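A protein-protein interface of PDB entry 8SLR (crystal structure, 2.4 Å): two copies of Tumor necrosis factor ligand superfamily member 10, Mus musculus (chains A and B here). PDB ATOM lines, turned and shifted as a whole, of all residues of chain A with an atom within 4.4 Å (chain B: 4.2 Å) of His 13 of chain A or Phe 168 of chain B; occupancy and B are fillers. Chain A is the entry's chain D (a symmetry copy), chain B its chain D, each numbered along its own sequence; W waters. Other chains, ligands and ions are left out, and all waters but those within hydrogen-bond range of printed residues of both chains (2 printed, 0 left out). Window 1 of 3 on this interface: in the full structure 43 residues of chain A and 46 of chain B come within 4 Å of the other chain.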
ATOM      1  N   ALA A  12      34.962  19.964 -12.588  1.00  0.00           N
ATOM      2  CA  ALA A  12      34.323  20.611 -11.457  1.00  0.00           C
ATOM      3  C   ALA A  12      33.380  19.615 -10.804  1.00  0.00           C
ATOM      4  O   ALA A  12      32.758  18.798 -11.487  1.00  0.00           O
ATOM      5  CB  ALA A  12      33.558  21.863 -11.893  1.00  0.00           C
ATOM      6  N   HIS A  13      33.292  19.685  -9.477  1.00  0.00           N
ATOM      7  CA  HIS A  13      32.267  18.974  -8.718  1.00  0.00           C
ATOM      8  C   HIS A  13      31.869  19.869  -7.556  1.00  0.00           C
ATOM      9  O   HIS A  13      32.708  20.179  -6.706  1.00  0.00           O
ATOM     10  CB  HIS A  13      32.782  17.621  -8.216  1.00  0.00           C
ATOM     11  CG  HIS A  13      31.804  16.864  -7.366  1.00  0.00           C
ATOM     12  ND1 HIS A  13      30.901  15.958  -7.885  1.00  0.00           N
ATOM     13  CD2 HIS A  13      31.604  16.863  -6.027  1.00  0.00           C
ATOM     14  CE1 HIS A  13      30.183  15.441  -6.902  1.00  0.00           C
ATOM     15  NE2 HIS A  13      30.588  15.975  -5.764  1.00  0.00           N
ATOM     16  N   ILE A  14      30.615  20.306  -7.537  1.00  0.00           N
ATOM     17  CA  ILE A  14      30.096  21.167  -6.482  1.00  0.00           C
ATOM     18  C   ILE A  14      28.912  20.462  -5.831  1.00  0.00           C
ATOM     19  O   ILE A  14      28.215  19.666  -6.469  1.00  0.00           O
ATOM     20  CB  ILE A  14      29.728  22.562  -7.034  1.00  0.00           C
ATOM     21  CG1 ILE A  14      28.502  22.528  -7.961  1.00  0.00           C
ATOM     22  CG2 ILE A  14      30.917  23.116  -7.798  1.00  0.00           C
ATOM     23  CD1 ILE A  14      28.209  23.879  -8.654  1.00  0.00           C
ATOM     24  N   THR A  15      28.704  20.747  -4.543  1.00  0.00           N
ATOM     25  CA  THR A  15      27.771  20.006  -3.700  1.00  0.00           C
ATOM     26  C   THR A  15      26.813  20.960  -3.002  1.00  0.00           C
ATOM     27  O   THR A  15      27.073  22.160  -2.873  1.00  0.00           O
ATOM     28  CB  THR A  15      28.502  19.191  -2.618  1.00  0.00           C
ATOM     29  OG1 THR A  15      29.055  20.086  -1.643  1.00  0.00           O
ATOM     30  CG2 THR A  15      29.621  18.350  -3.216  1.00  0.00           C
ATOM     31  N   MET A 117      29.121   9.917  -1.570  1.00  0.00           N
ATOM     32  CA  MET A 117      27.874  10.017  -2.314  1.00  0.00           C
ATOM     33  C   MET A 117      26.825   9.130  -1.658  1.00  0.00           C
ATOM     34  O   MET A 117      27.127   8.016  -1.222  1.00  0.00           O
ATOM     35  CB  MET A 117      28.049   9.599  -3.783  1.00  0.00           C
ATOM     36  CG  MET A 117      28.918  10.519  -4.616  1.00  0.00           C
ATOM     37  SD  MET A 117      29.195   9.825  -6.264  1.00  0.00           S
ATOM     38  CE  MET A 117      30.544   8.686  -5.927  1.00  0.00           C
ATOM     39  N   GLY A 139      27.049   8.499  -9.472  1.00  0.00           N
ATOM     40  CA  GLY A 139      28.477   8.668  -9.652  1.00  0.00           C
ATOM     41  C   GLY A 139      28.868  10.125  -9.551  1.00  0.00           C
ATOM     42  O   GLY A 139      28.019  11.021  -9.581  1.00  0.00           O
ATOM     43  N   LEU A 141      32.718  12.963  -9.249  1.00  0.00           N
ATOM     44  CA  LEU A 141      34.138  13.261  -9.377  1.00  0.00           C
ATOM     45  C   LEU A 141      34.715  13.594  -8.010  1.00  0.00           C
ATOM     46  O   LEU A 141      34.186  14.462  -7.308  1.00  0.00           O
ATOM     47  CB  LEU A 141      34.357  14.455 -10.301  1.00  0.00           C
ATOM     48  CG  LEU A 141      34.015  14.330 -11.771  1.00  0.00           C
ATOM     49  CD1 LEU A 141      34.035  15.700 -12.434  1.00  0.00           C
ATOM     50  CD2 LEU A 141      35.023  13.423 -12.407  1.00  0.00           C
ATOM     51  N   PHE A 142      35.797  12.911  -7.635  1.00  0.00           N
ATOM     52  CA  PHE A 142      36.418  13.115  -6.336  1.00  0.00           C
ATOM     53  C   PHE A 142      37.928  13.006  -6.468  1.00  0.00           C
ATOM     54  O   PHE A 142      38.438  12.178  -7.228  1.00  0.00           O
ATOM     55  CB  PHE A 142      35.872  12.108  -5.315  1.00  0.00           C
ATOM     56  CG  PHE A 142      34.429  12.332  -4.998  1.00  0.00           C
ATOM     57  CD1 PHE A 142      33.439  11.709  -5.737  1.00  0.00           C
ATOM     58  CD2 PHE A 142      34.058  13.222  -4.001  1.00  0.00           C
ATOM     59  CE1 PHE A 142      32.106  11.950  -5.476  1.00  0.00           C
ATOM     60  CE2 PHE A 142      32.727  13.463  -3.729  1.00  0.00           C
ATOM     61  CZ  PHE A 142      31.748  12.827  -4.464  1.00  0.00           C
ATOM     62  N   TRP B  42      25.195  25.997  -4.038  1.00  0.00           N
ATOM     63  CA  TRP B  42      26.248  25.013  -4.233  1.00  0.00           C
ATOM     64  C   TRP B  42      27.524  25.475  -3.536  1.00  0.00           C
ATOM     65  O   TRP B  42      27.841  26.669  -3.531  1.00  0.00           O
ATOM     66  CB  TRP B  42      26.559  24.813  -5.711  1.00  0.00           C
ATOM     67  CG  TRP B  42      25.472  24.305  -6.613  1.00  0.00           C
ATOM     68  CD1 TRP B  42      24.945  24.954  -7.683  1.00  0.00           C
ATOM     69  CD2 TRP B  42      24.836  23.020  -6.572  1.00  0.00           C
ATOM     70  NE1 TRP B  42      24.012  24.165  -8.307  1.00  0.00           N
ATOM     71  CE2 TRP B  42      23.928  22.971  -7.643  1.00  0.00           C
ATOM     72  CE3 TRP B  42      24.943  21.912  -5.730  1.00  0.00           C
ATOM     73  CZ2 TRP B  42      23.124  21.858  -7.891  1.00  0.00           C
ATOM     74  CZ3 TRP B  42      24.143  20.811  -5.976  1.00  0.00           C
ATOM     75  CH2 TRP B  42      23.251  20.790  -7.050  1.00  0.00           C
ATOM     76  N   HIS B  49      35.722  17.109  -1.096  1.00  0.00           N
ATOM     77  CA  HIS B  49      34.291  17.063  -1.367  1.00  0.00           C
ATOM     78  C   HIS B  49      33.894  17.837  -2.611  1.00  0.00           C
ATOM     79  O   HIS B  49      33.016  17.386  -3.345  1.00  0.00           O
ATOM     80  CB  HIS B  49      33.512  17.612  -0.161  1.00  0.00           C
ATOM     81  CG  HIS B  49      33.807  16.903   1.125  1.00  0.00           C
ATOM     82  ND1 HIS B  49      33.152  15.754   1.510  1.00  0.00           N
ATOM     83  CD2 HIS B  49      34.688  17.181   2.115  1.00  0.00           C
ATOM     84  CE1 HIS B  49      33.614  15.357   2.683  1.00  0.00           C
ATOM     85  NE2 HIS B  49      34.546  16.206   3.072  1.00  0.00           N
ATOM     86  N   SER B  50      34.515  18.987  -2.869  1.00  0.00           N
ATOM     87  CA  SER B  50      34.202  19.787  -4.046  1.00  0.00           C
ATOM     88  C   SER B  50      35.453  20.514  -4.519  1.00  0.00           C
ATOM     89  O   SER B  50      36.415  20.698  -3.766  1.00  0.00           O
ATOM     90  CB  SER B  50      33.083  20.793  -3.757  1.00  0.00           C
ATOM     91  OG  SER B  50      33.362  21.525  -2.584  1.00  0.00           O
ATOM     92  N   PHE B  51      35.428  20.933  -5.785  1.00  0.00           N
ATOM     93  CA  PHE B  51      36.598  21.537  -6.410  1.00  0.00           C
ATOM     94  C   PHE B  51      36.184  22.180  -7.725  1.00  0.00           C
ATOM     95  O   PHE B  51      35.172  21.807  -8.328  1.00  0.00           O
ATOM     96  CB  PHE B  51      37.705  20.499  -6.662  1.00  0.00           C
ATOM     97  CG  PHE B  51      37.372  19.532  -7.763  1.00  0.00           C
ATOM     98  CD1 PHE B  51      36.631  18.399  -7.499  1.00  0.00           C
ATOM     99  CD2 PHE B  51      37.780  19.769  -9.067  1.00  0.00           C
ATOM    100  CE1 PHE B  51      36.302  17.527  -8.511  1.00  0.00           C
ATOM    101  CE2 PHE B  51      37.443  18.901 -10.075  1.00  0.00           C
ATOM    102  CZ  PHE B  51      36.706  17.782  -9.798  1.00  0.00           C
ATOM    103  N   TYR B  73      26.917  16.040 -15.293  1.00  0.00           N
ATOM    104  CA  TYR B  73      26.042  15.215 -14.467  1.00  0.00           C
ATOM    105  C   TYR B  73      25.540  16.012 -13.274  1.00  0.00           C
ATOM    106  O   TYR B  73      26.155  16.994 -12.851  1.00  0.00           O
ATOM    107  CB  TYR B  73      26.759  13.958 -13.962  1.00  0.00           C
ATOM    108  CG  TYR B  73      27.927  14.291 -13.074  1.00  0.00           C
ATOM    109  CD1 TYR B  73      29.160  14.588 -13.622  1.00  0.00           C
ATOM    110  CD2 TYR B  73      27.795  14.327 -11.693  1.00  0.00           C
ATOM    111  CE1 TYR B  73      30.220  14.909 -12.835  1.00  0.00           C
ATOM    112  CE2 TYR B  73      28.860  14.648 -10.894  1.00  0.00           C
ATOM    113  CZ  TYR B  73      30.066  14.938 -11.476  1.00  0.00           C
ATOM    114  OH  TYR B  73      31.140  15.269 -10.703  1.00  0.00           O
ATOM    115  N   SER B  74      24.424  15.551 -12.714  1.00  0.00           N
ATOM    116  CA  SER B  74      23.923  16.095 -11.463  1.00  0.00           C
ATOM    117  C   SER B  74      23.105  15.037 -10.741  1.00  0.00           C
ATOM    118  O   SER B  74      22.400  14.246 -11.376  1.00  0.00           O
ATOM    119  CB  SER B  74      23.067  17.340 -11.707  1.00  0.00           C
ATOM    120  OG  SER B  74      22.493  17.797 -10.496  1.00  0.00           O
ATOM    121  N   GLN B  75      23.210  15.022  -9.415  1.00  0.00           N
ATOM    122  CA  GLN B  75      22.294  14.271  -8.572  1.00  0.00           C
ATOM    123  C   GLN B  75      21.517  15.262  -7.723  1.00  0.00           C
ATOM    124  O   GLN B  75      22.097  16.207  -7.182  1.00  0.00           O
ATOM    125  CB  GLN B  75      23.006  13.242  -7.675  1.00  0.00           C
ATOM    126  CG  GLN B  75      22.003  12.313  -6.968  1.00  0.00           C
ATOM    127  CD  GLN B  75      22.599  10.981  -6.523  1.00  0.00           C
ATOM    128  OE1 GLN B  75      22.247   9.919  -7.040  1.00  0.00           O
ATOM    129  NE2 GLN B  75      23.480  11.032  -5.547  1.00  0.00           N
ATOM    130  N   GLU B 165      26.325  15.182   0.535  1.00  0.00           N
ATOM    131  CA  GLU B 165      26.518  13.801   0.116  1.00  0.00           C
ATOM    132  C   GLU B 165      25.539  13.419  -0.981  1.00  0.00           C
ATOM    133  O   GLU B 165      25.855  12.576  -1.827  1.00  0.00           O
ATOM    134  CB  GLU B 165      26.333  12.859   1.313  1.00  0.00           C
ATOM    135  CG  GLU B 165      27.142  13.205   2.566  1.00  0.00           C
ATOM    136  CD  GLU B 165      26.746  12.358   3.771  1.00  0.00           C
ATOM    137  OE1 GLU B 165      25.742  11.617   3.685  1.00  0.00           O
ATOM    138  OE2 GLU B 165      27.440  12.434   4.811  1.00  0.00           O
ATOM    139  N   SER B 167      23.303  15.636  -3.006  1.00  0.00           N
ATOM    140  CA  SER B 167      22.969  16.554  -4.086  1.00  0.00           C
ATOM    141  C   SER B 167      24.243  17.229  -4.559  1.00  0.00           C
ATOM    142  O   SER B 167      24.967  17.825  -3.756  1.00  0.00           O
ATOM    143  CB  SER B 167      21.951  17.598  -3.627  1.00  0.00           C
ATOM    144  OG  SER B 167      20.702  16.985  -3.362  1.00  0.00           O
ATOM    145  N   PHE B 168      24.515  17.136  -5.858  1.00  0.00           N
ATOM    146  CA  PHE B 168      25.750  17.675  -6.403  1.00  0.00           C
ATOM    147  C   PHE B 168      25.605  17.825  -7.910  1.00  0.00           C
ATOM    148  O   PHE B 168      24.619  17.393  -8.515  1.00  0.00           O
ATOM    149  CB  PHE B 168      26.955  16.794  -6.036  1.00  0.00           C
ATOM    150  CG  PHE B 168      26.747  15.323  -6.295  1.00  0.00           C
ATOM    151  CD1 PHE B 168      26.776  14.808  -7.585  1.00  0.00           C
ATOM    152  CD2 PHE B 168      26.546  14.449  -5.243  1.00  0.00           C
ATOM    153  CE1 PHE B 168      26.596  13.461  -7.814  1.00  0.00           C
ATOM    154  CE2 PHE B 168      26.366  13.104  -5.468  1.00  0.00           C
ATOM    155  CZ  PHE B 168      26.396  12.608  -6.757  1.00  0.00           C
ATOM    156  N   PHE B 169      26.641  18.404  -8.511  1.00  0.00           N
ATOM    157  CA  PHE B 169      26.604  18.894  -9.881  1.00  0.00           C
ATOM    158  C   PHE B 169      28.052  19.017 -10.329  1.00  0.00           C
ATOM    159  O   PHE B 169      28.862  19.615  -9.615  1.00  0.00           O
ATOM    160  CB  PHE B 169      25.864  20.243  -9.921  1.00  0.00           C
ATOM    161  CG  PHE B 169      25.894  20.967 -11.250  1.00  0.00           C
ATOM    162  CD1 PHE B 169      25.812  20.294 -12.460  1.00  0.00           C
ATOM    163  CD2 PHE B 169      25.930  22.354 -11.269  1.00  0.00           C
ATOM    164  CE1 PHE B 169      25.807  21.002 -13.666  1.00  0.00           C
ATOM    165  CE2 PHE B 169      25.928  23.059 -12.465  1.00  0.00           C
ATOM    166  CZ  PHE B 169      25.863  22.386 -13.658  1.00  0.00           C
ATOM    167  N   GLY B 170      28.389  18.420 -11.473  1.00  0.00           N
ATOM    168  CA  GLY B 170      29.766  18.465 -11.922  1.00  0.00           C
ATOM    169  C   GLY B 170      29.887  18.238 -13.410  1.00  0.00           C
ATOM    170  O   GLY B 170      28.909  17.969 -14.109  1.00  0.00           O
HETATM  171  O   HOH W   1      34.731  16.161  -5.387  1.00  0.00           O
HETATM  172  O   HOH W   2      31.464  20.553  -0.634  1.00  0.00           O
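Hydrophobic or aromatic side chains of chain B within 4 Å of the printed part of chain A: Trp 42, Phe 51, Tyr 73, Phe 168 and Phe 169. Printed residues of chain A that touch a printed residue of chain B: Ala 12, His 13, Ile 14, Thr 15, Met 117, Gly 139, Leu 141 and Phe 142. Among the printed residues, no Asp or Glu carboxylate lies within 4 Å of a Lys or Arg side-chain nitrogen of the other chain.
No position is printed for both chains. Of the 22 pairs that touch across the chains among the printed residues, none has its exchanged pair printed and touching as well.
His 13 of chain A touches just these residues of chain B: His 49, Ser 50, Phe 51, Tyr 73, Phe 168 and Phe 169. Of chain A, only His 13 (3.5 Å), Ile 14 (3.2 Å), Met 117 (3.7 Å) and Gly 139 (3.3 Å) come within 4 Å of Phe 168 of chain B. Of the printed residues of chain A, His 49 of chain B touches His 13, Thr 15 and Phe 142. Printed residues of chain B within 4 Å of Thr 15 of chain A: Trp 42 (3.3 Å), His 49 (3.5 Å) and Ser 167 (3.6 Å). Gln 75 of chain B touches none of the printed residues of chain A. Ser 74 of chain B touches none of the printed residues of chain A. The nearest residue of chain A that does not touch Phe 168 of chain B is Thr 15 of chain A (4.1 Å).
Phe 51 of chain B touches Ala 12 of chain A. Tyr 73 of chain B touches Ala 12 of chain A. His 49 of chain B touches His 13 of chain A. His 13 of chain A touches Ser 50 of chain B (O to CB, 3.0 Å). CE1 of His 13 of chain A touches CG of Phe 168 of chain B, 3.5 Å away. Thr 15 of chain A touches Trp 42 of chain B. Thr 15 of chain A touches His 49 of chain B (CG2 to O, 3.5 Å). Thr 15 of chain A touches Ser 167 of chain B. Met 117 of chain A touches Glu 165 of chain B. Phe 168 of chain B touches Met 117 of chain A (CE2 to CG, 3.7 Å).
Water W1 lies within hydrogen-bond range of O of Leu 141 of chain A (2.6 Å) and O of His 49 of chain B (2.9 Å). Water W2 bridges the side-chain hydroxyl of Thr 15 of chain A and the side-chain hydroxyl of Ser 50 of chain B.
N of Phe 51 of chain B sits at hydrogen-bond distance from O of His 13 of chain A (3.0 Å). A ring nitrogen (ND1) of His 13 of chain A lies within hydrogen-bond range of the side-chain hydroxyl of Tyr 73 of chain B (2.9 Å). The backbone NH of Leu 141 of chain A sits at hydrogen-bond distance from the side-chain hydroxyl of Tyr 73 of chain B. N of Ile 14 of chain A sits at hydrogen-bond distance from O of Phe 169 of chain B, at 2.8 Å.
The backbone carbonyl oxygen (O) of Tyr 73 of chain B lies within hydrogen-bond range of the backbone NH (N) of Gly 170 of chain B (3.0 Å). OG of Ser 74 of chain B sits at hydrogen-bond distance from O of Phe 168 of chain B, at 2.9 Å. The backbone NH (N) of Gln 75 of chain B is in hydrogen-bond range of the backbone carbonyl oxygen (O) of Phe 168 of chain B, 2.9 Å away.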
